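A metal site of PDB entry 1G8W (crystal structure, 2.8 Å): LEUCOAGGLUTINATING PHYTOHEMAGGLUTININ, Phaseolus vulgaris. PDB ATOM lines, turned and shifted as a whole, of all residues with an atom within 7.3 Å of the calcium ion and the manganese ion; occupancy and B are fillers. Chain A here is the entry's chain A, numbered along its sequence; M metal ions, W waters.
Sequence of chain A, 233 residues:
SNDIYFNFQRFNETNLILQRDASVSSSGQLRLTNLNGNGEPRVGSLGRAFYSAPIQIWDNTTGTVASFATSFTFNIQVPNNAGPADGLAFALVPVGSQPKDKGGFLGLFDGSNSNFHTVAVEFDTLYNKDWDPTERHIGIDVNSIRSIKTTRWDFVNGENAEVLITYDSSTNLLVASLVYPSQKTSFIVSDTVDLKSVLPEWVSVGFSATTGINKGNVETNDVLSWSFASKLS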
ATOM      1  N   ASP A  86      35.123  19.984  -9.764  1.00  0.00           N
ATOM      2  CA  ASP A  86      34.096  20.444 -10.696  1.00  0.00           C
ATOM      3  C   ASP A  86      32.697  20.218 -10.125  1.00  0.00           C
ATOM      4  O   ASP A  86      31.743  20.915 -10.473  1.00  0.00           O
ATOM      5  CB  ASP A  86      34.244  19.687 -12.014  1.00  0.00           C
ATOM      6  CG  ASP A  86      34.827  20.543 -13.125  1.00  0.00           C
ATOM      7  OD1 ASP A  86      34.110  21.436 -13.633  1.00  0.00           O
ATOM      8  OD2 ASP A  86      35.998  20.325 -13.482  1.00  0.00           O
ATOM      9  N   GLY A  87      32.566  19.223  -9.239  1.00  0.00           N
ATOM     10  CA  GLY A  87      31.275  18.933  -8.645  1.00  0.00           C
ATOM     11  C   GLY A  87      31.090  17.488  -8.231  1.00  0.00           C
ATOM     12  O   GLY A  87      31.977  16.639  -8.404  1.00  0.00           O
ATOM     13  N   GLY A 103      36.353  16.485 -15.427  1.00  0.00           N
ATOM     14  CA  GLY A 103      35.928  17.866 -15.236  1.00  0.00           C
ATOM     15  C   GLY A 103      34.440  18.173 -15.261  1.00  0.00           C
ATOM     16  O   GLY A 103      33.633  17.493 -14.629  1.00  0.00           O
ATOM     17  N   GLY A 104      34.072  19.210 -16.003  1.00  0.00           N
ATOM     18  CA  GLY A 104      32.688  19.621 -16.087  1.00  0.00           C
ATOM     19  C   GLY A 104      31.679  18.530 -16.414  1.00  0.00           C
ATOM     20  O   GLY A 104      30.487  18.705 -16.175  1.00  0.00           O
ATOM     21  N   PHE A 105      32.137  17.411 -16.962  1.00  0.00           N
ATOM     22  CA  PHE A 105      31.222  16.332 -17.298  1.00  0.00           C
ATOM     23  C   PHE A 105      30.900  15.423 -16.108  1.00  0.00           C
ATOM     24  O   PHE A 105      30.109  14.480 -16.235  1.00  0.00           O
ATOM     25  CB  PHE A 105      31.791  15.528 -18.457  1.00  0.00           C
ATOM     26  CG  PHE A 105      31.622  16.205 -19.773  1.00  0.00           C
ATOM     27  CD1 PHE A 105      30.349  16.406 -20.298  1.00  0.00           C
ATOM     28  CD2 PHE A 105      32.720  16.678 -20.481  1.00  0.00           C
ATOM     29  CE1 PHE A 105      30.180  17.077 -21.507  1.00  0.00           C
ATOM     30  CE2 PHE A 105      32.557  17.342 -21.689  1.00  0.00           C
ATOM     31  CZ  PHE A 105      31.286  17.535 -22.203  1.00  0.00           C
ATOM     32  N   LEU A 106      31.511  15.714 -14.971  1.00  0.00           N
ATOM     33  CA  LEU A 106      31.271  14.961 -13.746  1.00  0.00           C
ATOM     34  C   LEU A 106      31.432  13.438 -13.856  1.00  0.00           C
ATOM     35  O   LEU A 106      30.966  12.698 -12.990  1.00  0.00           O
ATOM     36  CB  LEU A 106      29.888  15.310 -13.228  1.00  0.00           C
ATOM     37  CG  LEU A 106      29.656  16.814 -13.049  1.00  0.00           C
ATOM     38  CD1 LEU A 106      28.217  17.082 -12.623  1.00  0.00           C
ATOM     39  CD2 LEU A 106      30.622  17.333 -12.016  1.00  0.00           C
ATOM     40  N   GLU A 122      22.996  16.792  -9.871  1.00  0.00           N
ATOM     41  CA  GLU A 122      24.327  17.318  -9.678  1.00  0.00           C
ATOM     42  C   GLU A 122      24.436  18.473  -8.729  1.00  0.00           C
ATOM     43  O   GLU A 122      23.490  19.227  -8.512  1.00  0.00           O
ATOM     44  CB  GLU A 122      24.908  17.766 -11.014  1.00  0.00           C
ATOM     45  CG  GLU A 122      24.070  18.831 -11.677  1.00  0.00           C
ATOM     46  CD  GLU A 122      24.758  19.429 -12.862  1.00  0.00           C
ATOM     47  OE1 GLU A 122      25.182  18.663 -13.749  1.00  0.00           O
ATOM     48  OE2 GLU A 122      24.882  20.670 -12.913  1.00  0.00           O
ATOM     49  N   PHE A 123      25.627  18.597  -8.157  1.00  0.00           N
ATOM     50  CA  PHE A 123      25.964  19.685  -7.250  1.00  0.00           C
ATOM     51  C   PHE A 123      27.206  20.314  -7.869  1.00  0.00           C
ATOM     52  O   PHE A 123      28.337  20.042  -7.488  1.00  0.00           O
ATOM     53  CB  PHE A 123      26.210  19.132  -5.851  1.00  0.00           C
ATOM     54  CG  PHE A 123      25.019  18.429  -5.286  1.00  0.00           C
ATOM     55  CD1 PHE A 123      24.789  17.081  -5.572  1.00  0.00           C
ATOM     56  CD2 PHE A 123      24.060  19.131  -4.556  1.00  0.00           C
ATOM     57  CE1 PHE A 123      23.614  16.443  -5.144  1.00  0.00           C
ATOM     58  CE2 PHE A 123      22.872  18.508  -4.131  1.00  0.00           C
ATOM     59  CZ  PHE A 123      22.652  17.168  -4.423  1.00  0.00           C
ATOM     60  N   ASP A 124      26.925  21.144  -8.878  1.00  0.00           N
ATOM     61  CA  ASP A 124      27.897  21.862  -9.692  1.00  0.00           C
ATOM     62  C   ASP A 124      28.617  23.010  -8.983  1.00  0.00           C
ATOM     63  O   ASP A 124      27.997  23.979  -8.562  1.00  0.00           O
ATOM     64  CB  ASP A 124      27.180  22.423 -10.908  1.00  0.00           C
ATOM     65  CG  ASP A 124      28.058  22.489 -12.101  1.00  0.00           C
ATOM     66  OD1 ASP A 124      29.258  22.765 -11.928  1.00  0.00           O
ATOM     67  OD2 ASP A 124      27.533  22.263 -13.212  1.00  0.00           O
ATOM     68  N   THR A 125      29.934  22.920  -8.879  1.00  0.00           N
ATOM     69  CA  THR A 125      30.675  23.972  -8.204  1.00  0.00           C
ATOM     70  C   THR A 125      31.463  24.894  -9.138  1.00  0.00           C
ATOM     71  O   THR A 125      31.989  25.915  -8.692  1.00  0.00           O
ATOM     72  CB  THR A 125      31.657  23.373  -7.173  1.00  0.00           C
ATOM     73  OG1 THR A 125      32.428  22.345  -7.802  1.00  0.00           O
ATOM     74  CG2 THR A 125      30.893  22.805  -5.980  1.00  0.00           C
ATOM     75  N   LEU A 126      31.544  24.540 -10.416  1.00  0.00           N
ATOM     76  CA  LEU A 126      32.286  25.347 -11.390  1.00  0.00           C
ATOM     77  C   LEU A 126      31.447  25.726 -12.594  1.00  0.00           C
ATOM     78  O   LEU A 126      30.737  24.895 -13.160  1.00  0.00           O
ATOM     79  CB  LEU A 126      33.533  24.613 -11.858  1.00  0.00           C
ATOM     80  CG  LEU A 126      34.456  25.442 -12.764  1.00  0.00           C
ATOM     81  CD1 LEU A 126      34.916  26.704 -12.040  1.00  0.00           C
ATOM     82  CD2 LEU A 126      35.643  24.588 -13.171  1.00  0.00           C
ATOM     83  N   TYR A 127      31.562  26.994 -12.998  1.00  0.00           N
ATOM     84  CA  TYR A 127      30.807  27.512 -14.136  1.00  0.00           C
ATOM     85  C   TYR A 127      31.373  27.102 -15.502  1.00  0.00           C
ATOM     86  O   TYR A 127      32.548  27.331 -15.780  1.00  0.00           O
ATOM     87  CB  TYR A 127      30.747  29.050 -14.053  1.00  0.00           C
ATOM     88  CG  TYR A 127      30.124  29.721 -15.256  1.00  0.00           C
ATOM     89  CD1 TYR A 127      28.796  29.484 -15.610  1.00  0.00           C
ATOM     90  CD2 TYR A 127      30.886  30.551 -16.070  1.00  0.00           C
ATOM     91  CE1 TYR A 127      28.240  30.053 -16.746  1.00  0.00           C
ATOM     92  CE2 TYR A 127      30.334  31.135 -17.213  1.00  0.00           C
ATOM     93  CZ  TYR A 127      29.005  30.875 -17.549  1.00  0.00           C
ATOM     94  OH  TYR A 127      28.461  31.414 -18.684  1.00  0.00           O
ATOM     95  N   ASN A 128      30.551  26.492 -16.343  1.00  0.00           N
ATOM     96  CA  ASN A 128      30.967  26.091 -17.686  1.00  0.00           C
ATOM     97  C   ASN A 128      30.168  26.889 -18.705  1.00  0.00           C
ATOM     98  O   ASN A 128      28.998  26.599 -18.944  1.00  0.00           O
ATOM     99  CB  ASN A 128      30.712  24.597 -17.933  1.00  0.00           C
ATOM    100  CG  ASN A 128      31.485  23.708 -16.986  1.00  0.00           C
ATOM    101  OD1 ASN A 128      31.034  23.431 -15.875  1.00  0.00           O
ATOM    102  ND2 ASN A 128      32.655  23.263 -17.411  1.00  0.00           N
ATOM    103  N   TRP A 131      27.072  25.496 -21.079  1.00  0.00           N
ATOM    104  CA  TRP A 131      25.772  24.950 -20.664  1.00  0.00           C
ATOM    105  C   TRP A 131      25.317  25.264 -19.248  1.00  0.00           C
ATOM    106  O   TRP A 131      24.146  25.074 -18.932  1.00  0.00           O
ATOM    107  CB  TRP A 131      25.816  23.422 -20.827  1.00  0.00           C
ATOM    108  CG  TRP A 131      26.887  22.769 -19.974  1.00  0.00           C
ATOM    109  CD1 TRP A 131      26.923  22.710 -18.599  1.00  0.00           C
ATOM    110  CD2 TRP A 131      28.106  22.161 -20.419  1.00  0.00           C
ATOM    111  NE1 TRP A 131      28.077  22.104 -18.181  1.00  0.00           N
ATOM    112  CE2 TRP A 131      28.828  21.764 -19.269  1.00  0.00           C
ATOM    113  CE3 TRP A 131      28.663  21.911 -21.685  1.00  0.00           C
ATOM    114  CZ2 TRP A 131      30.078  21.126 -19.342  1.00  0.00           C
ATOM    115  CZ3 TRP A 131      29.907  21.281 -21.760  1.00  0.00           C
ATOM    116  CH2 TRP A 131      30.593  20.897 -20.590  1.00  0.00           C
ATOM    117  N   ASP A 132      26.220  25.721 -18.393  1.00  0.00           N
ATOM    118  CA  ASP A 132      25.877  26.007 -17.003  1.00  0.00           C
ATOM    119  C   ASP A 132      25.328  27.390 -16.738  1.00  0.00           C
ATOM    120  O   ASP A 132      25.640  28.337 -17.446  1.00  0.00           O
ATOM    121  CB  ASP A 132      27.104  25.847 -16.084  1.00  0.00           C
ATOM    122  CG  ASP A 132      27.294  24.437 -15.574  1.00  0.00           C
ATOM    123  OD1 ASP A 132      26.309  23.685 -15.452  1.00  0.00           O
ATOM    124  OD2 ASP A 132      28.453  24.079 -15.267  1.00  0.00           O
ATOM    125  N   PRO A 133      24.470  27.520 -15.710  1.00  0.00           N
ATOM    126  CA  PRO A 133      23.915  28.823 -15.360  1.00  0.00           C
ATOM    127  C   PRO A 133      25.099  29.580 -14.725  1.00  0.00           C
ATOM    128  O   PRO A 133      26.119  28.961 -14.399  1.00  0.00           O
ATOM    129  CB  PRO A 133      22.808  28.481 -14.363  1.00  0.00           C
ATOM    130  CG  PRO A 133      23.228  27.185 -13.800  1.00  0.00           C
ATOM    131  CD  PRO A 133      23.750  26.451 -15.001  1.00  0.00           C
ATOM    132  N   GLU A 135      25.663  30.994 -11.694  1.00  0.00           N
ATOM    133  CA  GLU A 135      26.052  30.703 -10.323  1.00  0.00           C
ATOM    134  C   GLU A 135      26.083  29.207 -10.018  1.00  0.00           C
ATOM    135  O   GLU A 135      25.507  28.405 -10.746  1.00  0.00           O
ATOM    136  CB  GLU A 135      25.116  31.406  -9.360  1.00  0.00           C
ATOM    137  CG  GLU A 135      24.991  32.899  -9.614  1.00  0.00           C
ATOM    138  CD  GLU A 135      24.333  33.637  -8.473  1.00  0.00           C
ATOM    139  OE1 GLU A 135      24.987  33.815  -7.417  1.00  0.00           O
ATOM    140  OE2 GLU A 135      23.155  34.026  -8.613  1.00  0.00           O
ATOM    141  N   HIS A 137      25.143  25.731  -8.633  1.00  0.00           N
ATOM    142  CA  HIS A 137      23.776  25.246  -8.546  1.00  0.00           C
ATOM    143  C   HIS A 137      23.587  23.754  -8.277  1.00  0.00           C
ATOM    144  O   HIS A 137      24.525  22.965  -8.244  1.00  0.00           O
ATOM    145  CB  HIS A 137      23.128  25.549  -9.882  1.00  0.00           C
ATOM    146  CG  HIS A 137      23.981  25.134 -11.037  1.00  0.00           C
ATOM    147  ND1 HIS A 137      25.127  25.814 -11.397  1.00  0.00           N
ATOM    148  CD2 HIS A 137      23.933  24.047 -11.850  1.00  0.00           C
ATOM    149  CE1 HIS A 137      25.751  25.164 -12.360  1.00  0.00           C
ATOM    150  NE2 HIS A 137      25.053  24.081 -12.649  1.00  0.00           N
ATOM    151  N   ILE A 138      22.315  23.406  -8.111  1.00  0.00           N
ATOM    152  CA  ILE A 138      21.883  22.033  -7.938  1.00  0.00           C
ATOM    153  C   ILE A 138      21.085  21.844  -9.229  1.00  0.00           C
ATOM    154  O   ILE A 138      20.273  22.701  -9.583  1.00  0.00           O
ATOM    155  CB  ILE A 138      20.929  21.886  -6.760  1.00  0.00           C
ATOM    156  CG1 ILE A 138      21.649  22.262  -5.467  1.00  0.00           C
ATOM    157  CG2 ILE A 138      20.442  20.451  -6.657  1.00  0.00           C
ATOM    158  CD1 ILE A 138      20.744  22.272  -4.244  1.00  0.00           C
ATOM    159  N   GLY A 139      21.338  20.751  -9.955  1.00  0.00           N
ATOM    160  CA  GLY A 139      20.609  20.539 -11.191  1.00  0.00           C
ATOM    161  C   GLY A 139      20.163  19.122 -11.435  1.00  0.00           C
ATOM    162  O   GLY A 139      20.825  18.167 -10.995  1.00  0.00           O
ATOM    163  N   ASP A 141      19.826  16.396 -14.081  1.00  0.00           N
ATOM    164  CA  ASP A 141      20.350  16.039 -15.403  1.00  0.00           C
ATOM    165  C   ASP A 141      19.700  14.789 -15.991  1.00  0.00           C
ATOM    166  O   ASP A 141      19.747  13.715 -15.390  1.00  0.00           O
ATOM    167  CB  ASP A 141      21.856  15.783 -15.334  1.00  0.00           C
ATOM    168  CG  ASP A 141      22.620  16.963 -14.786  1.00  0.00           C
ATOM    169  OD1 ASP A 141      22.004  18.022 -14.590  1.00  0.00           O
ATOM    170  OD2 ASP A 141      23.829  16.819 -14.556  1.00  0.00           O
ATOM    171  N   ILE A 145      24.737  16.873 -19.682  1.00  0.00           N
ATOM    172  CA  ILE A 145      25.397  17.628 -18.628  1.00  0.00           C
ATOM    173  C   ILE A 145      24.663  18.974 -18.487  1.00  0.00           C
ATOM    174  O   ILE A 145      24.858  19.689 -17.510  1.00  0.00           O
ATOM    175  CB  ILE A 145      26.888  17.838 -18.954  1.00  0.00           C
ATOM    176  CG1 ILE A 145      27.639  18.325 -17.703  1.00  0.00           C
ATOM    177  CG2 ILE A 145      27.043  18.845 -20.076  1.00  0.00           C
ATOM    178  CD1 ILE A 145      27.655  17.333 -16.571  1.00  0.00           C
ATOM    179  N   ARG A 146      23.832  19.313 -19.468  1.00  0.00           N
ATOM    180  CA  ARG A 146      23.048  20.539 -19.444  1.00  0.00           C
ATOM    181  C   ARG A 146      21.753  20.239 -18.693  1.00  0.00           C
ATOM    182  O   ARG A 146      20.822  19.686 -19.257  1.00  0.00           O
ATOM    183  CB  ARG A 146      22.696  20.998 -20.859  1.00  0.00           C
ATOM    184  N   SER A 147      21.700  20.615 -17.423  1.00  0.00           N
ATOM    185  CA  SER A 147      20.539  20.355 -16.577  1.00  0.00           C
ATOM    186  C   SER A 147      19.218  20.808 -17.168  1.00  0.00           C
ATOM    187  O   SER A 147      19.107  21.888 -17.738  1.00  0.00           O
ATOM    188  CB  SER A 147      20.728  20.998 -15.214  1.00  0.00           C
ATOM    189  OG  SER A 147      21.955  20.593 -14.642  1.00  0.00           O
ATOM    190  N   THR A 150      17.508  23.936 -12.859  1.00  0.00           N
ATOM    191  CA  THR A 150      18.440  24.135 -11.754  1.00  0.00           C
ATOM    192  C   THR A 150      17.919  25.106 -10.699  1.00  0.00           C
ATOM    193  O   THR A 150      16.795  25.617 -10.796  1.00  0.00           O
ATOM    194  CB  THR A 150      19.800  24.704 -12.251  1.00  0.00           C
ATOM    195  OG1 THR A 150      19.611  26.049 -12.693  1.00  0.00           O
ATOM    196  CG2 THR A 150      20.352  23.876 -13.387  1.00  0.00           C
HETATM  197 CA    CA M   1      30.025  22.775 -13.967  1.00  0.00          CA
HETATM  198 MN    MN M   2      25.379  22.235 -13.908  1.00  0.00          MN
HETATM  199  O   HOH W   1      23.825  22.389 -15.308  1.00  0.00           O
HETATM  200  O   HOH W   2      26.516  20.744 -15.135  1.00  0.00           O
HETATM  201  O   HOH W   3      31.697  21.199 -13.430  1.00  0.00           O
HETATM  202  O   HOH W   4      29.352  20.796 -15.024  1.00  0.00           O
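OG of Ser 147 touches the manganese ion, 3.9 Å away.
Five residues have an atom within 4 Å of the manganese ion: Glu 122, Asp 124, Asp 132, His 137 and Ser 147.
The side-chain carboxylate (OD1) of Asp 124 binds the calcium ion (2.2 Å).
The side-chain amide oxygen (OD1) of Asn 128 binds the calcium ion, at 2.3 Å.
Water W4 binds the calcium ion, 2.3 Å away.
Water W3 binds the calcium ion, at 2.4 Å.
The backbone carbonyl oxygen (O) of Leu 126 is bound to the calcium ion (2.4 Å).
The calcium ion is bound by OD2 of Asp 132 (2.4 Å).
OD2 of Asp 124 is bound to the calcium ion, 2.7 Å away.
OE2 of Glu 122 binds the manganese ion, 1.9 Å away.
The manganese ion is bound by water W1 (2.1 Å).
Water W2 is bound to the manganese ion (2.2 Å).
A ring nitrogen (NE2) of His 137 binds the manganese ion (2.3 Å).
The manganese ion is bound by OD2 of Asp 124 (2.3 Å).
The manganese ion is bound by OD1 of Asp 132 (2.3 Å).
A ring nitrogen (ND1) of His 137 sits at hydrogen-bond distance from the backbone carbonyl oxygen (O) of Glu 135 (2.7 Å).
OG of Ser 147 lies within hydrogen-bond range of OD1 of Asp 141 (2.6 Å).
The side-chain carboxylate of Glu 122 lies close to the side-chain carboxylate of Asp 141.
The backbone NH (N) of Glu 122 is in hydrogen-bond range of the backbone carbonyl oxygen (O) of Gly 139 (2.8 Å).
The side-chain carboxylate (OE2) of Glu 122 sits close to the side-chain hydroxyl (OG) of Ser 147 (3.4 Å).
Water W2 bridges the side-chain carboxylate of Glu 122 and the backbone carbonyl oxygen of Ile 145.
Within 4 Å of the calcium ion: Asp 124, Leu 126, Asn 128 and Asp 132.
The nearest printed residue that does not touch the calcium ion is Asp 86 (4.3 Å).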
